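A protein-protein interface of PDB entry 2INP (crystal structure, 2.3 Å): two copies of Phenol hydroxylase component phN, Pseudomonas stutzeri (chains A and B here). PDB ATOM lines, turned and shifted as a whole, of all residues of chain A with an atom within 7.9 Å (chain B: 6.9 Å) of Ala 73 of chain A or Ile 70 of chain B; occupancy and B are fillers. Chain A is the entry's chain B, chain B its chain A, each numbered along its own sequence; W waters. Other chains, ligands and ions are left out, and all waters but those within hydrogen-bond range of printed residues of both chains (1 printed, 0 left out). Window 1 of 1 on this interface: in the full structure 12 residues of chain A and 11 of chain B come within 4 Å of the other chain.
The side-chain hydroxyl (OG1) of Thr 219 of chain B lies within hydrogen-bond range of the backbone carbonyl oxygen (O) of Met 215 of chain B.
The side-chain amide nitrogen of Asn 77 of chain A sits at hydrogen-bond distance from the backbone carbonyl oxygen of Ala 73 of chain A, 2.8 Å away.
N of Gly 79 of chain A lies within hydrogen-bond range of O of Phe 74 of chain A (2.8 Å).
Among the printed residues, pairs that only touch across the chains: Asn 77 of chain A with Val 218 of chain B (3.1 Å), Ala 73 of chain A with Met 215 of chain B (3.5 Å), Ala 69 of chain A with Ile 70 of chain B (3.6 Å), Ala 73 of chain A with Ile 70 of chain B (3.6 Å), Phe 74 of chain A with Met 215 of chain B (3.7 Å), Ile 70 of chain A with Ala 73 of chain B (3.8 Å), Ile 70 of chain A with Ala 69 of chain B (3.8 Å), Lys 66 of chain A with Ala 69 of chain B (3.8 Å), Ala 69 of chain A with Lys 66 of chain B (3.8 Å), Asn 77 of chain A with Met 215 of chain B (3.8 Å) and Met 215 of chain A with Met 215 of chain B (3.9 Å).
Of the printed residues of chain B, Lys 66 of chain A touches Ala 69.
Printed residues of chain B within 4 Å of Ala 69 of chain A: Lys 66 and Ile 70.
Of the printed residues of chain B, Asn 77 of chain A touches Met 215 and Val 218.
Of the printed residues of chain B, Met 215 of chain A touches Met 215 (3.9 Å).
Printed residues of chain A within 4 Å of Ala 69 of chain B: Lys 66 and Ile 70.
Asp 72 of chain B touches none of the printed residues of chain A.
Of the printed residues of chain A, Met 215 of chain B touches Ala 73, Phe 74, Asn 77 and Met 215.
Ala 216 of chain B touches none of the printed residues of chain A.
The nearest residue of chain B that does not touch Ala 73 of chain A is Thr 219 of chain B (4.7 Å).
The nearest residue of chain A that does not touch Ile 70 of chain B is Ile 70 of chain A (4.3 Å).
Of the 17 printed residues of chain B, 6 touch a printed residue of chain A.
Hydrophobic or aromatic side chains of chain B that line the printed part of chain A: Ala 69, Ile 70, Ala 73, Met 215 and Val 218.
Along chain B the printed residues that touch a printed residue of chain A span positions 66 to 218.
Hydrophobic or aromatic side chains of chain A within 4 Å of the printed part of chain B: Ala 69, Ile 70, Ala 73 and Met 215.
Among the printed residues, no Asp or Glu carboxylate lies within 4 Å of a Lys or Arg side-chain nitrogen of the other chain.
Lys 66 of chain A touches Ala 69 of chain B, and with the chains exchanged Ala 69 of chain A touches Lys 66 of chain B.
Ala 69 of chain A touches Ile 70 of chain B, and with the chains exchanged Ile 70 of chain A touches Ala 69 of chain B.
Ala 73 of chain A touches Met 215 of chain B, but with the chains exchanged Met 215 of chain A does not touch Ala 73 of chain B (4.1 Å).
Met 215 of chain A touches its own counterpart, Met 215 of chain B.
13 positions are printed for both chains.
Of the 11 pairs that touch across the chains among the printed residues, 7 have their exchanged pair printed and touching as well.
Water W1 lies within hydrogen-bond range of OG1 of Thr 219 of chain B (2.8 Å) and ND2 of Asn 77 of chain A (2.9 Å).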
ATOM      1  N   LYS A  65      -3.883   6.888  11.666  1.00  0.00           N
ATOM      2  CA  LYS A  65      -4.289   5.680  12.303  1.00  0.00           C
ATOM      3  C   LYS A  65      -4.131   4.497  11.333  1.00  0.00           C
ATOM      4  O   LYS A  65      -3.609   3.459  11.711  1.00  0.00           O
ATOM      5  CB  LYS A  65      -5.712   5.851  12.775  1.00  0.00           C
ATOM      6  CG  LYS A  65      -6.239   4.651  13.544  1.00  0.00           C
ATOM      7  CD  LYS A  65      -7.578   4.934  14.167  1.00  0.00           C
ATOM      8  CE  LYS A  65      -7.526   6.244  14.975  1.00  0.00           C
ATOM      9  NZ  LYS A  65      -8.315   6.113  16.219  1.00  0.00           N
ATOM     10  N   LYS A  66      -4.595   4.662  10.088  1.00  0.00           N
ATOM     11  CA  LYS A  66      -4.433   3.628   9.070  1.00  0.00           C
ATOM     12  C   LYS A  66      -2.977   3.321   8.697  1.00  0.00           C
ATOM     13  O   LYS A  66      -2.612   2.183   8.619  1.00  0.00           O
ATOM     14  CB  LYS A  66      -5.239   3.982   7.789  1.00  0.00           C
ATOM     15  CG  LYS A  66      -6.706   4.191   8.083  1.00  0.00           C
ATOM     16  CD  LYS A  66      -7.492   3.909   6.858  1.00  0.00           C
ATOM     17  CE  LYS A  66      -7.386   4.999   5.910  1.00  0.00           C
ATOM     18  NZ  LYS A  66      -8.682   5.614   5.959  1.00  0.00           N
ATOM     19  N   LEU A  67      -2.156   4.354   8.533  1.00  0.00           N
ATOM     20  CA  LEU A  67      -0.730   4.223   8.257  1.00  0.00           C
ATOM     21  C   LEU A  67       0.020   3.384   9.330  1.00  0.00           C
ATOM     22  O   LEU A  67       0.671   2.343   9.003  1.00  0.00           O
ATOM     23  CB  LEU A  67      -0.149   5.630   8.129  1.00  0.00           C
ATOM     24  CG  LEU A  67       1.326   5.750   7.693  1.00  0.00           C
ATOM     25  CD1 LEU A  67       1.451   5.051   6.358  1.00  0.00           C
ATOM     26  CD2 LEU A  67       1.689   7.168   7.470  1.00  0.00           C
ATOM     27  N   TYR A  68      -0.131   3.758  10.611  1.00  0.00           N
ATOM     28  CA  TYR A  68       0.568   3.033  11.686  1.00  0.00           C
ATOM     29  C   TYR A  68       0.076   1.601  11.860  1.00  0.00           C
ATOM     30  O   TYR A  68       0.847   0.687  12.180  1.00  0.00           O
ATOM     31  CB  TYR A  68       0.621   3.853  12.980  1.00  0.00           C
ATOM     32  CG  TYR A  68       1.635   4.974  12.884  1.00  0.00           C
ATOM     33  CD1 TYR A  68       2.960   4.754  13.226  1.00  0.00           C
ATOM     34  CD2 TYR A  68       1.304   6.180  12.299  1.00  0.00           C
ATOM     35  CE1 TYR A  68       3.944   5.760  13.081  1.00  0.00           C
ATOM     36  CE2 TYR A  68       2.241   7.189  12.136  1.00  0.00           C
ATOM     37  CZ  TYR A  68       3.586   6.954  12.517  1.00  0.00           C
ATOM     38  OH  TYR A  68       4.511   7.940  12.411  1.00  0.00           O
ATOM     39  N   ALA A  69      -1.181   1.348  11.536  1.00  0.00           N
ATOM     40  CA  ALA A  69      -1.659  -0.059  11.641  1.00  0.00           C
ATOM     41  C   ALA A  69      -0.937  -0.814  10.562  1.00  0.00           C
ATOM     42  O   ALA A  69      -0.615  -1.938  10.697  1.00  0.00           O
ATOM     43  CB  ALA A  69      -3.235  -0.141  11.398  1.00  0.00           C
ATOM     44  N   ILE A  70      -0.711  -0.193   9.432  1.00  0.00           N
ATOM     45  CA  ILE A  70      -0.042  -0.915   8.322  1.00  0.00           C
ATOM     46  C   ILE A  70       1.421  -1.137   8.611  1.00  0.00           C
ATOM     47  O   ILE A  70       1.888  -2.205   8.377  1.00  0.00           O
ATOM     48  CB  ILE A  70      -0.283  -0.202   6.974  1.00  0.00           C
ATOM     49  CG1 ILE A  70      -1.763  -0.341   6.575  1.00  0.00           C
ATOM     50  CG2 ILE A  70       0.611  -0.805   5.862  1.00  0.00           C
ATOM     51  CD1 ILE A  70      -2.206   0.783   5.502  1.00  0.00           C
ATOM     52  N   PHE A  71       2.121  -0.108   9.128  1.00  0.00           N
ATOM     53  CA  PHE A  71       3.513  -0.191   9.560  1.00  0.00           C
ATOM     54  C   PHE A  71       3.679  -1.285  10.640  1.00  0.00           C
ATOM     55  O   PHE A  71       4.588  -2.118  10.554  1.00  0.00           O
ATOM     56  CB  PHE A  71       3.895   1.124  10.222  1.00  0.00           C
ATOM     57  CG  PHE A  71       4.167   2.261   9.265  1.00  0.00           C
ATOM     58  CD1 PHE A  71       4.228   2.038   7.846  1.00  0.00           C
ATOM     59  CD2 PHE A  71       4.393   3.563   9.780  1.00  0.00           C
ATOM     60  CE1 PHE A  71       4.560   3.049   6.989  1.00  0.00           C
ATOM     61  CE2 PHE A  71       4.710   4.638   8.890  1.00  0.00           C
ATOM     62  CZ  PHE A  71       4.813   4.367   7.492  1.00  0.00           C
ATOM     63  N   ASP A  72       2.816  -1.255  11.679  1.00  0.00           N
ATOM     64  CA  ASP A  72       2.817  -2.298  12.728  1.00  0.00           C
ATOM     65  C   ASP A  72       2.649  -3.692  12.140  1.00  0.00           C
ATOM     66  O   ASP A  72       3.351  -4.618  12.572  1.00  0.00           O
ATOM     67  CB  ASP A  72       1.722  -2.071  13.809  1.00  0.00           C
ATOM     68  CG  ASP A  72       1.987  -0.815  14.689  1.00  0.00           C
ATOM     69  OD1 ASP A  72       1.045  -0.358  15.394  1.00  0.00           O
ATOM     70  OD2 ASP A  72       3.120  -0.269  14.685  1.00  0.00           O
ATOM     71  N   ALA A  73       1.717  -3.844  11.195  1.00  0.00           N
ATOM     72  CA  ALA A  73       1.472  -5.154  10.576  1.00  0.00           C
ATOM     73  C   ALA A  73       2.631  -5.609   9.688  1.00  0.00           C
ATOM     74  O   ALA A  73       3.028  -6.780   9.766  1.00  0.00           O
ATOM     75  CB  ALA A  73       0.149  -5.164   9.767  1.00  0.00           C
ATOM     76  N   PHE A  74       3.161  -4.708   8.843  1.00  0.00           N
ATOM     77  CA  PHE A  74       4.375  -4.982   8.119  1.00  0.00           C
ATOM     78  C   PHE A  74       5.544  -5.501   8.995  1.00  0.00           C
ATOM     79  O   PHE A  74       6.236  -6.454   8.665  1.00  0.00           O
ATOM     80  CB  PHE A  74       4.788  -3.691   7.414  1.00  0.00           C
ATOM     81  CG  PHE A  74       5.960  -3.839   6.489  1.00  0.00           C
ATOM     82  CD1 PHE A  74       5.764  -4.270   5.160  1.00  0.00           C
ATOM     83  CD2 PHE A  74       7.264  -3.581   6.942  1.00  0.00           C
ATOM     84  CE1 PHE A  74       6.888  -4.400   4.277  1.00  0.00           C
ATOM     85  CE2 PHE A  74       8.376  -3.700   6.062  1.00  0.00           C
ATOM     86  CZ  PHE A  74       8.165  -4.130   4.763  1.00  0.00           C
ATOM     87  N   ALA A  75       5.774  -4.860  10.130  1.00  0.00           N
ATOM     88  CA  ALA A  75       6.853  -5.290  11.037  1.00  0.00           C
ATOM     89  C   ALA A  75       6.603  -6.676  11.645  1.00  0.00           C
ATOM     90  O   ALA A  75       7.475  -7.553  11.575  1.00  0.00           O
ATOM     91  CB  ALA A  75       7.088  -4.265  12.116  1.00  0.00           C
ATOM     92  N   GLN A  76       5.375  -6.884  12.167  1.00  0.00           N
ATOM     93  CA  GLN A  76       4.984  -8.099  12.899  1.00  0.00           C
ATOM     94  C   GLN A  76       5.087  -9.255  11.955  1.00  0.00           C
ATOM     95  O   GLN A  76       5.438 -10.396  12.308  1.00  0.00           O
ATOM     96  CB  GLN A  76       3.531  -7.941  13.388  1.00  0.00           C
ATOM     97  CG  GLN A  76       3.334  -8.297  14.901  1.00  0.00           C
ATOM     98  CD  GLN A  76       3.303  -9.797  15.088  1.00  0.00           C
ATOM     99  OE1 GLN A  76       3.995 -10.369  15.963  1.00  0.00           O
ATOM    100  NE2 GLN A  76       2.534 -10.471  14.214  1.00  0.00           N
ATOM    101  N   ASN A  77       4.790  -8.953  10.718  1.00  0.00           N
ATOM    102  CA  ASN A  77       4.769  -9.986   9.728  1.00  0.00           C
ATOM    103  C   ASN A  77       6.096 -10.091   8.943  1.00  0.00           C
ATOM    104  O   ASN A  77       6.187 -10.873   8.006  1.00  0.00           O
ATOM    105  CB  ASN A  77       3.537  -9.796   8.835  1.00  0.00           C
ATOM    106  CG  ASN A  77       2.218 -10.106   9.630  1.00  0.00           C
ATOM    107  OD1 ASN A  77       1.999 -11.291   9.972  1.00  0.00           O
ATOM    108  ND2 ASN A  77       1.436  -9.038  10.054  1.00  0.00           N
ATOM    109  N   ASN A  78       7.126  -9.338   9.348  1.00  0.00           N
ATOM    110  CA  ASN A  78       8.429  -9.418   8.583  1.00  0.00           C
ATOM    111  C   ASN A  78       8.274  -9.136   7.093  1.00  0.00           C
ATOM    112  O   ASN A  78       8.754  -9.882   6.261  1.00  0.00           O
ATOM    113  CB  ASN A  78       9.189 -10.718   8.892  1.00  0.00           C
ATOM    114  CG  ASN A  78       9.720 -10.714  10.350  1.00  0.00           C
ATOM    115  OD1 ASN A  78      10.341  -9.716  10.816  1.00  0.00           O
ATOM    116  ND2 ASN A  78       9.423 -11.773  11.097  1.00  0.00           N
ATOM    117  N   GLY A  79       7.533  -8.079   6.760  1.00  0.00           N
ATOM    118  CA  GLY A  79       7.265  -7.833   5.359  1.00  0.00           C
ATOM    119  C   GLY A  79       8.505  -7.446   4.565  1.00  0.00           C
ATOM    120  O   GLY A  79       8.440  -7.374   3.333  1.00  0.00           O
ATOM    121  N   HIS A 146      11.963  -0.714  10.323  1.00  0.00           N
ATOM    122  CA  HIS A 146      12.063  -2.150  10.294  1.00  0.00           C
ATOM    123  C   HIS A 146      13.162  -2.605   9.318  1.00  0.00           C
ATOM    124  O   HIS A 146      13.837  -3.591   9.565  1.00  0.00           O
ATOM    125  CB  HIS A 146      10.716  -2.784   9.897  1.00  0.00           C
ATOM    126  CG  HIS A 146      10.673  -4.270  10.069  1.00  0.00           C
ATOM    127  ND1 HIS A 146      10.725  -4.884  11.313  1.00  0.00           N
ATOM    128  CD2 HIS A 146      10.589  -5.268   9.152  1.00  0.00           C
ATOM    129  CE1 HIS A 146      10.709  -6.193  11.140  1.00  0.00           C
ATOM    130  NE2 HIS A 146      10.600  -6.454   9.846  1.00  0.00           N
ATOM    131  N   MET A 215       5.490  -2.879   0.961  1.00  0.00           N
ATOM    132  CA  MET A 215       4.275  -2.350   1.449  1.00  0.00           C
ATOM    133  C   MET A 215       4.489  -1.122   2.325  1.00  0.00           C
ATOM    134  O   MET A 215       3.743  -0.167   2.240  1.00  0.00           O
ATOM    135  CB  MET A 215       3.527  -3.430   2.215  1.00  0.00           C
ATOM    136  CG  MET A 215       2.228  -2.897   2.807  1.00  0.00           C
ATOM    137  SD  MET A 215       1.327  -4.157   3.732  1.00  0.00           S
ATOM    138  CE  MET A 215       1.020  -5.522   2.548  1.00  0.00           C
ATOM    139  N   GLU B  64     -11.566  -2.271  14.422  1.00  0.00           N
ATOM    140  CA  GLU B  64     -12.038  -2.498  13.039  1.00  0.00           C
ATOM    141  C   GLU B  64     -11.340  -1.527  12.074  1.00  0.00           C
ATOM    142  O   GLU B  64     -10.996  -1.932  10.990  1.00  0.00           O
ATOM    143  CB  GLU B  64     -13.582  -2.351  12.938  1.00  0.00           C
ATOM    144  CG  GLU B  64     -14.348  -3.482  13.560  1.00  0.00           C
ATOM    145  CD  GLU B  64     -14.379  -4.720  12.695  1.00  0.00           C
ATOM    146  OE1 GLU B  64     -13.656  -5.719  12.927  1.00  0.00           O
ATOM    147  OE2 GLU B  64     -15.160  -4.718  11.728  1.00  0.00           O
ATOM    148  N   LYS B  65     -11.140  -0.272  12.461  1.00  0.00           N
ATOM    149  CA  LYS B  65     -10.401   0.664  11.629  1.00  0.00           C
ATOM    150  C   LYS B  65      -9.024   0.167  11.259  1.00  0.00           C
ATOM    151  O   LYS B  65      -8.658   0.290  10.114  1.00  0.00           O
ATOM    152  CB  LYS B  65     -10.267   2.066  12.233  1.00  0.00           C
ATOM    153  CG  LYS B  65     -11.571   2.788  12.201  1.00  0.00           C
ATOM    154  CD  LYS B  65     -11.583   4.087  13.058  1.00  0.00           C
ATOM    155  CE  LYS B  65     -13.069   4.601  13.200  1.00  0.00           C
ATOM    156  NZ  LYS B  65     -13.244   5.226  14.516  1.00  0.00           N
ATOM    157  N   LYS B  66      -8.310  -0.417  12.224  1.00  0.00           N
ATOM    158  CA  LYS B  66      -6.986  -1.000  12.006  1.00  0.00           C
ATOM    159  C   LYS B  66      -7.034  -2.255  11.137  1.00  0.00           C
ATOM    160  O   LYS B  66      -6.182  -2.388  10.274  1.00  0.00           O
ATOM    161  CB  LYS B  66      -6.264  -1.356  13.306  1.00  0.00           C
ATOM    162  CG  LYS B  66      -5.926  -0.161  14.137  1.00  0.00           C
ATOM    163  CD  LYS B  66      -5.242  -0.574  15.534  1.00  0.00           C
ATOM    164  CE  LYS B  66      -5.315   0.650  16.460  1.00  0.00           C
ATOM    165  NZ  LYS B  66      -5.224   0.373  17.978  1.00  0.00           N
ATOM    166  N   LEU B  67      -8.003  -3.156  11.392  1.00  0.00           N
ATOM    167  CA  LEU B  67      -8.158  -4.356  10.650  1.00  0.00           C
ATOM    168  C   LEU B  67      -8.411  -4.049   9.131  1.00  0.00           C
ATOM    169  O   LEU B  67      -7.771  -4.650   8.285  1.00  0.00           O
ATOM    170  CB  LEU B  67      -9.272  -5.187  11.228  1.00  0.00           C
ATOM    171  CG  LEU B  67      -9.635  -6.519  10.579  1.00  0.00           C
ATOM    172  CD1 LEU B  67      -8.443  -7.469  10.627  1.00  0.00           C
ATOM    173  CD2 LEU B  67     -10.738  -7.179  11.444  1.00  0.00           C
ATOM    174  N   TYR B  68      -9.347  -3.126   8.815  1.00  0.00           N
ATOM    175  CA  TYR B  68      -9.717  -2.895   7.407  1.00  0.00           C
ATOM    176  C   TYR B  68      -8.610  -2.097   6.723  1.00  0.00           C
ATOM    177  O   TYR B  68      -8.390  -2.294   5.533  1.00  0.00           O
ATOM    178  CB  TYR B  68     -11.127  -2.244   7.253  1.00  0.00           C
ATOM    179  CG  TYR B  68     -12.206  -3.321   7.397  1.00  0.00           C
ATOM    180  CD1 TYR B  68     -12.686  -4.019   6.302  1.00  0.00           C
ATOM    181  CD2 TYR B  68     -12.694  -3.673   8.664  1.00  0.00           C
ATOM    182  CE1 TYR B  68     -13.639  -5.044   6.453  1.00  0.00           C
ATOM    183  CE2 TYR B  68     -13.631  -4.713   8.817  1.00  0.00           C
ATOM    184  CZ  TYR B  68     -14.111  -5.381   7.694  1.00  0.00           C
ATOM    185  OH  TYR B  68     -15.017  -6.419   7.842  1.00  0.00           O
ATOM    186  N   ALA B  69      -7.860  -1.265   7.467  1.00  0.00           N
ATOM    187  CA  ALA B  69      -6.675  -0.550   6.871  1.00  0.00           C
ATOM    188  C   ALA B  69      -5.724  -1.597   6.295  1.00  0.00           C
ATOM    189  O   ALA B  69      -5.214  -1.438   5.179  1.00  0.00           O
ATOM    190  CB  ALA B  69      -5.895   0.266   7.936  1.00  0.00           C
ATOM    191  N   ILE B  70      -5.427  -2.619   7.106  1.00  0.00           N
ATOM    192  CA  ILE B  70      -4.631  -3.758   6.733  1.00  0.00           C
ATOM    193  C   ILE B  70      -5.211  -4.626   5.589  1.00  0.00           C
ATOM    194  O   ILE B  70      -4.425  -5.057   4.606  1.00  0.00           O
ATOM    195  CB  ILE B  70      -4.258  -4.602   7.997  1.00  0.00           C
ATOM    196  CG1 ILE B  70      -3.432  -3.706   8.948  1.00  0.00           C
ATOM    197  CG2 ILE B  70      -3.388  -5.805   7.665  1.00  0.00           C
ATOM    198  CD1 ILE B  70      -3.328  -4.262  10.396  1.00  0.00           C
ATOM    199  N   PHE B  71      -6.526  -4.908   5.661  1.00  0.00           N
ATOM    200  CA  PHE B  71      -7.150  -5.741   4.625  1.00  0.00           C
ATOM    201  C   PHE B  71      -6.947  -4.947   3.333  1.00  0.00           C
ATOM    202  O   PHE B  71      -6.657  -5.524   2.370  1.00  0.00           O
ATOM    203  CB  PHE B  71      -8.650  -5.969   4.869  1.00  0.00           C
ATOM    204  CG  PHE B  71      -9.011  -7.065   5.888  1.00  0.00           C
ATOM    205  CD1 PHE B  71      -8.055  -7.940   6.432  1.00  0.00           C
ATOM    206  CD2 PHE B  71     -10.344  -7.197   6.287  1.00  0.00           C
ATOM    207  CE1 PHE B  71      -8.430  -8.901   7.347  1.00  0.00           C
ATOM    208  CE2 PHE B  71     -10.719  -8.122   7.182  1.00  0.00           C
ATOM    209  CZ  PHE B  71      -9.763  -9.001   7.702  1.00  0.00           C
ATOM    210  N   ASP B  72      -7.168  -3.632   3.329  1.00  0.00           N
ATOM    211  CA  ASP B  72      -7.051  -2.831   2.135  1.00  0.00           C
ATOM    212  C   ASP B  72      -5.584  -2.752   1.612  1.00  0.00           C
ATOM    213  O   ASP B  72      -5.359  -2.763   0.379  1.00  0.00           O
ATOM    214  CB  ASP B  72      -7.431  -1.375   2.365  1.00  0.00           C
ATOM    215  CG  ASP B  72      -8.923  -1.136   2.693  1.00  0.00           C
ATOM    216  OD1 ASP B  72      -9.077  -0.112   3.438  1.00  0.00           O
ATOM    217  OD2 ASP B  72      -9.880  -1.890   2.299  1.00  0.00           O
ATOM    218  N   ALA B  73      -4.610  -2.681   2.536  1.00  0.00           N
ATOM    219  CA  ALA B  73      -3.227  -2.635   2.125  1.00  0.00           C
ATOM    220  C   ALA B  73      -2.886  -3.983   1.528  1.00  0.00           C
ATOM    221  O   ALA B  73      -2.237  -4.035   0.513  1.00  0.00           O
ATOM    222  CB  ALA B  73      -2.266  -2.230   3.270  1.00  0.00           C
ATOM    223  N   PHE B  74      -3.243  -5.071   2.186  1.00  0.00           N
ATOM    224  CA  PHE B  74      -2.948  -6.399   1.668  1.00  0.00           C
ATOM    225  C   PHE B  74      -3.490  -6.590   0.232  1.00  0.00           C
ATOM    226  O   PHE B  74      -2.803  -7.124  -0.605  1.00  0.00           O
ATOM    227  CB  PHE B  74      -3.572  -7.410   2.625  1.00  0.00           C
ATOM    228  CG  PHE B  74      -3.486  -8.803   2.203  1.00  0.00           C
ATOM    229  CD1 PHE B  74      -2.401  -9.591   2.577  1.00  0.00           C
ATOM    230  CD2 PHE B  74      -4.502  -9.364   1.426  1.00  0.00           C
ATOM    231  CE1 PHE B  74      -2.350 -10.941   2.178  1.00  0.00           C
ATOM    232  CE2 PHE B  74      -4.459 -10.689   1.082  1.00  0.00           C
ATOM    233  CZ  PHE B  74      -3.409 -11.465   1.461  1.00  0.00           C
ATOM    234  N   ALA B  75      -4.708  -6.159  -0.028  1.00  0.00           N
ATOM    235  CA  ALA B  75      -5.337  -6.373  -1.308  1.00  0.00           C
ATOM    236  C   ALA B  75      -4.613  -5.482  -2.382  1.00  0.00           C
ATOM    237  O   ALA B  75      -4.317  -5.935  -3.437  1.00  0.00           O
ATOM    238  CB  ALA B  75      -6.820  -5.997  -1.246  1.00  0.00           C
ATOM    239  N   GLN B  76      -4.361  -4.234  -2.043  1.00  0.00           N
ATOM    240  CA  GLN B  76      -3.611  -3.283  -2.830  1.00  0.00           C
ATOM    241  C   GLN B  76      -2.157  -3.698  -3.215  1.00  0.00           C
ATOM    242  O   GLN B  76      -1.647  -3.316  -4.289  1.00  0.00           O
ATOM    243  CB  GLN B  76      -3.628  -1.967  -2.082  1.00  0.00           C
ATOM    244  CG  GLN B  76      -2.919  -0.807  -2.734  1.00  0.00           C
ATOM    245  CD  GLN B  76      -2.837   0.415  -1.740  1.00  0.00           C
ATOM    246  OE1 GLN B  76      -3.786   0.692  -0.953  1.00  0.00           O
ATOM    247  NE2 GLN B  76      -1.715   1.153  -1.800  1.00  0.00           N
ATOM    248  N   MET B 215      -0.706 -12.497   5.817  1.00  0.00           N
ATOM    249  CA  MET B 215      -0.958 -11.344   6.627  1.00  0.00           C
ATOM    250  C   MET B 215      -2.493 -11.070   6.913  1.00  0.00           C
ATOM    251  O   MET B 215      -2.858 -10.545   7.991  1.00  0.00           O
ATOM    252  CB  MET B 215      -0.285 -10.121   5.977  1.00  0.00           C
ATOM    253  CG  MET B 215      -0.470  -8.815   6.721  1.00  0.00           C
ATOM    254  SD  MET B 215      -0.022  -7.294   5.816  1.00  0.00           S
ATOM    255  CE  MET B 215       1.556  -7.237   6.609  1.00  0.00           C
ATOM    256  N   ALA B 216      -3.352 -11.330   5.916  1.00  0.00           N
ATOM    257  CA  ALA B 216      -4.782 -11.064   6.066  1.00  0.00           C
ATOM    258  C   ALA B 216      -5.340 -11.943   7.216  1.00  0.00           C
ATOM    259  O   ALA B 216      -5.857 -11.428   8.120  1.00  0.00           O
ATOM    260  CB  ALA B 216      -5.562 -11.282   4.756  1.00  0.00           C
ATOM    261  N   VAL B 218      -3.724 -13.724   9.605  1.00  0.00           N
ATOM    262  CA  VAL B 218      -3.055 -13.499  10.859  1.00  0.00           C
ATOM    263  C   VAL B 218      -3.544 -12.230  11.492  1.00  0.00           C
ATOM    264  O   VAL B 218      -3.784 -12.188  12.686  1.00  0.00           O
ATOM    265  CB  VAL B 218      -1.470 -13.567  10.741  1.00  0.00           C
ATOM    266  CG1 VAL B 218      -0.860 -12.167  10.690  1.00  0.00           C
ATOM    267  CG2 VAL B 218      -0.975 -14.312  11.956  1.00  0.00           C
ATOM    268  N   THR B 219      -3.785 -11.221  10.660  1.00  0.00           N
ATOM    269  CA  THR B 219      -4.345  -9.995  11.140  1.00  0.00           C
ATOM    270  C   THR B 219      -5.768 -10.198  11.740  1.00  0.00           C
ATOM    271  O   THR B 219      -6.067  -9.640  12.802  1.00  0.00           O
ATOM    272  CB  THR B 219      -4.263  -8.888  10.053  1.00  0.00           C
ATOM    273  OG1 THR B 219      -2.872  -8.718   9.637  1.00  0.00           O
ATOM    274  CG2 THR B 219      -4.807  -7.569  10.574  1.00  0.00           C
HETATM  275  O   HOH W   1      -0.904  -8.409  11.590  1.00  0.00           O
